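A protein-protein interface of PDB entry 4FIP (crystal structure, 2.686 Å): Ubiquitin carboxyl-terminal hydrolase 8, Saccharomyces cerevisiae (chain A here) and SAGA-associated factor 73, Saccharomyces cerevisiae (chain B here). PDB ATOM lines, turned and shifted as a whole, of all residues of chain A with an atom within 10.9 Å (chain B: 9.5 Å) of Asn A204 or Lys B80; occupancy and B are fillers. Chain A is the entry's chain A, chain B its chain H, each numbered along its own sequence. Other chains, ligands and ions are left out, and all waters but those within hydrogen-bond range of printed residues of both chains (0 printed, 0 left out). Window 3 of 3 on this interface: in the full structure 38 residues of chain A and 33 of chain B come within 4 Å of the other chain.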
ATOM      1  N   LYS A 194      21.164   1.918  18.834  1.00  0.00           N
ATOM      2  CA  LYS A 194      20.858   1.910  20.250  1.00  0.00           C
ATOM      3  C   LYS A 194      19.472   1.313  20.537  1.00  0.00           C
ATOM      4  O   LYS A 194      19.294   0.566  21.535  1.00  0.00           O
ATOM      5  CB  LYS A 194      20.973   3.330  20.828  1.00  0.00           C
ATOM      6  CG  LYS A 194      20.782   3.380  22.344  1.00  0.00           C
ATOM      7  CD  LYS A 194      21.596   4.481  23.025  1.00  0.00           C
ATOM      8  CE  LYS A 194      21.754   4.215  24.518  1.00  0.00           C
ATOM      9  NZ  LYS A 194      22.838   3.230  24.782  1.00  0.00           N
ATOM     10  N   HIS A 197      19.958  -2.449  20.517  1.00  0.00           N
ATOM     11  CA  HIS A 197      20.662  -2.837  21.732  1.00  0.00           C
ATOM     12  C   HIS A 197      19.682  -2.872  22.899  1.00  0.00           C
ATOM     13  O   HIS A 197      19.564  -3.878  23.574  1.00  0.00           O
ATOM     14  CB  HIS A 197      21.810  -1.834  21.891  1.00  0.00           C
ATOM     15  CG  HIS A 197      22.707  -2.032  23.090  1.00  0.00           C
ATOM     16  ND1 HIS A 197      23.903  -1.421  23.168  1.00  0.00           N
ATOM     17  CD2 HIS A 197      22.561  -2.785  24.283  1.00  0.00           C
ATOM     18  CE1 HIS A 197      24.501  -1.757  24.342  1.00  0.00           C
ATOM     19  NE2 HIS A 197      23.678  -2.595  25.019  1.00  0.00           N
ATOM     20  N   GLU A 198      18.908  -1.813  23.124  1.00  0.00           N
ATOM     21  CA  GLU A 198      17.895  -1.840  24.210  1.00  0.00           C
ATOM     22  C   GLU A 198      16.861  -2.927  24.032  1.00  0.00           C
ATOM     23  O   GLU A 198      16.467  -3.566  24.994  1.00  0.00           O
ATOM     24  CB  GLU A 198      17.174  -0.508  24.340  1.00  0.00           C
ATOM     25  CG  GLU A 198      18.083   0.581  24.885  1.00  0.00           C
ATOM     26  CD  GLU A 198      17.459   1.965  24.881  1.00  0.00           C
ATOM     27  OE1 GLU A 198      16.965   2.420  23.810  1.00  0.00           O
ATOM     28  OE2 GLU A 198      17.500   2.609  25.957  1.00  0.00           O
ATOM     29  N   TYR A 200      16.982  -5.826  22.078  1.00  0.00           N
ATOM     30  CA  TYR A 200      17.431  -7.213  21.988  1.00  0.00           C
ATOM     31  C   TYR A 200      18.539  -7.563  23.021  1.00  0.00           C
ATOM     32  O   TYR A 200      18.549  -8.658  23.558  1.00  0.00           O
ATOM     33  CB  TYR A 200      17.892  -7.509  20.565  1.00  0.00           C
ATOM     34  CG  TYR A 200      16.785  -7.665  19.531  1.00  0.00           C
ATOM     35  CD1 TYR A 200      16.176  -8.898  19.295  1.00  0.00           C
ATOM     36  CD2 TYR A 200      16.395  -6.584  18.745  1.00  0.00           C
ATOM     37  CE1 TYR A 200      15.187  -9.028  18.334  1.00  0.00           C
ATOM     38  CE2 TYR A 200      15.422  -6.713  17.773  1.00  0.00           C
ATOM     39  CZ  TYR A 200      14.822  -7.924  17.560  1.00  0.00           C
ATOM     40  OH  TYR A 200      13.850  -7.999  16.581  1.00  0.00           O
ATOM     41  N   GLY A 201      19.445  -6.630  23.300  1.00  0.00           N
ATOM     42  CA  GLY A 201      20.542  -6.876  24.208  1.00  0.00           C
ATOM     43  C   GLY A 201      20.210  -6.581  25.662  1.00  0.00           C
ATOM     44  O   GLY A 201      19.193  -7.056  26.185  1.00  0.00           O
ATOM     45  N   ALA A 202      21.077  -5.779  26.290  1.00  0.00           N
ATOM     46  CA  ALA A 202      21.098  -5.592  27.744  1.00  0.00           C
ATOM     47  C   ALA A 202      21.505  -4.187  28.221  1.00  0.00           C
ATOM     48  O   ALA A 202      21.873  -3.319  27.432  1.00  0.00           O
ATOM     49  CB  ALA A 202      22.019  -6.628  28.356  1.00  0.00           C
ATOM     50  N   LEU A 203      21.453  -4.002  29.541  1.00  0.00           N
ATOM     51  CA  LEU A 203      21.692  -2.692  30.205  1.00  0.00           C
ATOM     52  C   LEU A 203      23.200  -2.374  30.524  1.00  0.00           C
ATOM     53  O   LEU A 203      23.798  -1.510  29.871  1.00  0.00           O
ATOM     54  CB  LEU A 203      20.822  -2.584  31.490  1.00  0.00           C
ATOM     55  CG  LEU A 203      19.308  -2.902  31.452  1.00  0.00           C
ATOM     56  CD1 LEU A 203      19.015  -4.403  31.543  1.00  0.00           C
ATOM     57  CD2 LEU A 203      18.588  -2.153  32.568  1.00  0.00           C
ATOM     58  N   ASN A 204      23.787  -3.055  31.520  1.00  0.00           N
ATOM     59  CA  ASN A 204      25.205  -2.880  31.933  1.00  0.00           C
ATOM     60  C   ASN A 204      25.744  -1.442  31.883  1.00  0.00           C
ATOM     61  O   ASN A 204      25.213  -0.530  32.531  1.00  0.00           O
ATOM     62  CB  ASN A 204      26.110  -3.802  31.105  1.00  0.00           C
ATOM     63  CG  ASN A 204      25.937  -5.272  31.465  1.00  0.00           C
ATOM     64  OD1 ASN A 204      25.571  -6.103  30.625  1.00  0.00           O
ATOM     65  ND2 ASN A 204      26.192  -5.596  32.727  1.00  0.00           N
ATOM     66  N   THR A 215      16.445   3.172  32.306  1.00  0.00           N
ATOM     67  CA  THR A 215      16.130   1.752  32.476  1.00  0.00           C
ATOM     68  C   THR A 215      14.821   1.349  31.762  1.00  0.00           C
ATOM     69  O   THR A 215      14.456   0.167  31.706  1.00  0.00           O
ATOM     70  CB  THR A 215      16.089   1.348  33.974  1.00  0.00           C
ATOM     71  OG1 THR A 215      15.952  -0.081  34.093  1.00  0.00           O
ATOM     72  CG2 THR A 215      14.947   2.070  34.724  1.00  0.00           C
ATOM     73  N   ARG A 217      13.344   0.994  28.091  1.00  0.00           N
ATOM     74  CA  ARG A 217      14.043   0.765  26.842  1.00  0.00           C
ATOM     75  C   ARG A 217      13.591   1.857  25.887  1.00  0.00           C
ATOM     76  O   ARG A 217      12.977   1.597  24.861  1.00  0.00           O
ATOM     77  CB  ARG A 217      13.725  -0.621  26.306  1.00  0.00           C
ATOM     78  CG  ARG A 217      14.334  -1.737  27.116  1.00  0.00           C
ATOM     79  CD  ARG A 217      13.803  -3.080  26.656  1.00  0.00           C
ATOM     80  NE  ARG A 217      12.412  -3.239  27.056  1.00  0.00           N
ATOM     81  CZ  ARG A 217      12.012  -3.665  28.250  1.00  0.00           C
ATOM     82  NH1 ARG A 217      12.889  -3.997  29.186  1.00  0.00           N
ATOM     83  NH2 ARG A 217      10.724  -3.774  28.512  1.00  0.00           N
ATOM     84  N   VAL B  77      24.781 -12.021  23.433  1.00  0.00           N
ATOM     85  CA  VAL B  77      24.874 -10.699  24.024  1.00  0.00           C
ATOM     86  C   VAL B  77      26.202 -10.574  24.781  1.00  0.00           C
ATOM     87  O   VAL B  77      26.548 -11.460  25.547  1.00  0.00           O
ATOM     88  CB  VAL B  77      23.681 -10.444  24.958  1.00  0.00           C
ATOM     89  CG1 VAL B  77      23.901  -9.146  25.736  1.00  0.00           C
ATOM     90  CG2 VAL B  77      22.391 -10.416  24.149  1.00  0.00           C
ATOM     91  N   CYS B  78      26.943  -9.487  24.528  1.00  0.00           N
ATOM     92  CA  CYS B  78      28.220  -9.196  25.213  1.00  0.00           C
ATOM     93  C   CYS B  78      28.018  -9.033  26.709  1.00  0.00           C
ATOM     94  O   CYS B  78      27.100  -8.333  27.129  1.00  0.00           O
ATOM     95  CB  CYS B  78      28.855  -7.917  24.651  1.00  0.00           C
ATOM     96  SG  CYS B  78      30.448  -7.515  25.400  1.00  0.00           S
ATOM     97  N   GLU B  79      28.867  -9.671  27.510  1.00  0.00           N
ATOM     98  CA  GLU B  79      28.733  -9.596  28.975  1.00  0.00           C
ATOM     99  C   GLU B  79      29.023  -8.194  29.453  1.00  0.00           C
ATOM    100  O   GLU B  79      28.431  -7.760  30.417  1.00  0.00           O
ATOM    101  CB  GLU B  79      29.683 -10.561  29.701  1.00  0.00           C
ATOM    102  CG  GLU B  79      29.384 -12.044  29.504  1.00  0.00           C
ATOM    103  CD  GLU B  79      28.275 -12.569  30.405  1.00  0.00           C
ATOM    104  OE1 GLU B  79      28.103 -13.804  30.494  1.00  0.00           O
ATOM    105  OE2 GLU B  79      27.569 -11.757  31.025  1.00  0.00           O
ATOM    106  N   LYS B  80      29.924  -7.484  28.778  1.00  0.00           N
ATOM    107  CA  LYS B  80      30.319  -6.151  29.231  1.00  0.00           C
ATOM    108  C   LYS B  80      29.507  -5.011  28.596  1.00  0.00           C
ATOM    109  O   LYS B  80      28.936  -4.208  29.329  1.00  0.00           O
ATOM    110  CB  LYS B  80      31.826  -5.937  29.032  1.00  0.00           C
ATOM    111  CG  LYS B  80      32.691  -6.595  30.109  1.00  0.00           C
ATOM    112  CD  LYS B  80      32.829  -8.107  29.916  1.00  0.00           C
ATOM    113  CE  LYS B  80      33.301  -8.830  31.185  1.00  0.00           C
ATOM    114  NZ  LYS B  80      33.167 -10.319  31.050  1.00  0.00           N
ATOM    115  N   CYS B  81      29.483  -4.943  27.256  1.00  0.00           N
ATOM    116  CA  CYS B  81      28.656  -3.987  26.480  1.00  0.00           C
ATOM    117  C   CYS B  81      27.192  -4.120  26.762  1.00  0.00           C
ATOM    118  O   CYS B  81      26.530  -3.119  26.929  1.00  0.00           O
ATOM    119  CB  CYS B  81      28.719  -4.244  24.963  1.00  0.00           C
ATOM    120  SG  CYS B  81      30.193  -3.718  24.105  1.00  0.00           S
ATOM    121  N   GLY B  82      26.689  -5.361  26.699  1.00  0.00           N
ATOM    122  CA  GLY B  82      25.243  -5.641  26.598  1.00  0.00           C
ATOM    123  C   GLY B  82      24.698  -5.696  25.170  1.00  0.00           C
ATOM    124  O   GLY B  82      23.528  -6.050  24.970  1.00  0.00           O
ATOM    125  N   LYS B  83      25.555  -5.359  24.190  1.00  0.00           N
ATOM    126  CA  LYS B  83      25.215  -5.329  22.768  1.00  0.00           C
ATOM    127  C   LYS B  83      24.836  -6.693  22.241  1.00  0.00           C
ATOM    128  O   LYS B  83      25.526  -7.661  22.547  1.00  0.00           O
ATOM    129  CB  LYS B  83      26.388  -4.804  21.931  1.00  0.00           C
ATOM    130  CG  LYS B  83      26.457  -3.265  21.848  1.00  0.00           C
ATOM    131  CD  LYS B  83      27.606  -2.830  20.943  1.00  0.00           C
ATOM    132  CE  LYS B  83      27.649  -1.333  20.645  1.00  0.00           C
ATOM    133  NZ  LYS B  83      27.856  -1.088  19.178  1.00  0.00           N
ATOM    134  N   PRO B  84      23.747  -6.786  21.442  1.00  0.00           N
ATOM    135  CA  PRO B  84      23.423  -8.051  20.823  1.00  0.00           C
ATOM    136  C   PRO B  84      24.309  -8.263  19.606  1.00  0.00           C
ATOM    137  O   PRO B  84      24.435  -7.367  18.779  1.00  0.00           O
ATOM    138  CB  PRO B  84      21.953  -7.895  20.424  1.00  0.00           C
ATOM    139  CG  PRO B  84      21.650  -6.434  20.490  1.00  0.00           C
ATOM    140  CD  PRO B  84      22.891  -5.719  20.928  1.00  0.00           C
ATOM    141  N   LEU B  85      24.931  -9.437  19.514  1.00  0.00           N
ATOM    142  CA  LEU B  85      25.897  -9.718  18.455  1.00  0.00           C
ATOM    143  C   LEU B  85      25.482 -10.889  17.579  1.00  0.00           C
ATOM    144  O   LEU B  85      25.131 -11.962  18.076  1.00  0.00           O
ATOM    145  CB  LEU B  85      27.283  -9.982  19.041  1.00  0.00           C
ATOM    146  CG  LEU B  85      27.888  -8.853  19.883  1.00  0.00           C
ATOM    147  CD1 LEU B  85      28.932  -9.397  20.876  1.00  0.00           C
ATOM    148  CD2 LEU B  85      28.465  -7.752  19.015  1.00  0.00           C
ATOM    149  N   HIS B  93      34.188  -8.405  17.841  1.00  0.00           N
ATOM    150  CA  HIS B  93      33.858  -7.546  18.954  1.00  0.00           C
ATOM    151  C   HIS B  93      34.836  -7.793  20.057  1.00  0.00           C
ATOM    152  O   HIS B  93      35.393  -6.832  20.621  1.00  0.00           O
ATOM    153  CB  HIS B  93      32.450  -7.805  19.428  1.00  0.00           C
ATOM    154  CG  HIS B  93      31.974  -6.827  20.443  1.00  0.00           C
ATOM    155  ND1 HIS B  93      31.770  -5.530  20.146  1.00  0.00           N
ATOM    156  CD2 HIS B  93      31.662  -6.982  21.805  1.00  0.00           C
ATOM    157  CE1 HIS B  93      31.344  -4.873  21.270  1.00  0.00           C
ATOM    158  NE2 HIS B  93      31.280  -5.769  22.281  1.00  0.00           N
ATOM    159  N   LEU B  94      35.076  -9.078  20.353  1.00  0.00           N
ATOM    160  CA  LEU B  94      35.984  -9.457  21.418  1.00  0.00           C
ATOM    161  C   LEU B  94      37.419  -9.137  21.064  1.00  0.00           C
ATOM    162  O   LEU B  94      38.152  -8.635  21.894  1.00  0.00           O
ATOM    163  CB  LEU B  94      35.903 -10.949  21.682  1.00  0.00           C
ATOM    164  CG  LEU B  94      34.535 -11.544  21.998  1.00  0.00           C
ATOM    165  CD1 LEU B  94      34.637 -13.053  22.192  1.00  0.00           C
ATOM    166  CD2 LEU B  94      33.931 -10.875  23.211  1.00  0.00           C
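A ring nitrogen (NE2) of His A197 lies within hydrogen-bond range of the backbone carbonyl oxygen of Cys B81 (3.5 Å). The backbone carbonyl oxygen of Gly B82 sits close to a ring nitrogen (NE2) of His A197 (3.5 Å). N of Lys B83 sits at hydrogen-bond distance from NE2 of His A197, 3.4 Å away. O of Gly B82 lies within hydrogen-bond range of N of Ala A202, at 2.8 Å. The side-chain amide oxygen of Asn A204 sits close to the backbone carbonyl oxygen of Glu B79, 3.3 Å away.
NE2 of His A197 sits at hydrogen-bond distance from O of Ala A202, at 3.1 Å. The backbone NH of Lys B80 sits close to the side-chain sulfur of Cys B78 (3.4 Å). N of Cys B78 is in hydrogen-bond range of O of Lys B83 (3.0 Å).
His A197 touches Pro B84. Tyr A200 touches Pro B84. Gly A201 touches Val B77. Gly A201 touches Gly B82. Gly A201 touches Pro B84 (N to CG, 3.6 Å). Lys B80 touches Asn A204 (O to CB, 3.4 Å).
Of the printed residues of chain B, His A197 touches Cys B81 (3.5 Å), Gly B82 (3.3 Å), Lys B83 (3.4 Å) and Pro B84 (3.7 Å). Printed residues of chain B within 4 Å of Ala A202: Gly B82. No residue of chain B comes within 4 Å of Leu A203. Printed residues of chain B within 4 Å of Asn A204: Glu B79 (3.3 Å) and Lys B80 (3.4 Å). Of the printed residues of chain A, Val B77 touches Gly A201 (3.99 Å). No residue of chain A comes within 4 Å of Cys B78. Printed residues of chain A within 4 Å of Lys B80: Asn A204. Of chain A, only His A197 comes within 4 Å of Cys B81. The nearest residue of chain B that does not touch Asn A204 is Gly B82 (4.1 Å). The nearest residue of chain A that does not touch Lys B80 is Leu A203 (5.8 Å).
Hydrophobic or aromatic side chains of chain A that line the printed part of chain B: His A197, Tyr A200 and Ala A202. Printed residues of chain B that touch a printed residue of chain A: Val B77, Glu B79, Lys B80, Cys B81, Gly B82, Lys B83 and Pro B84.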
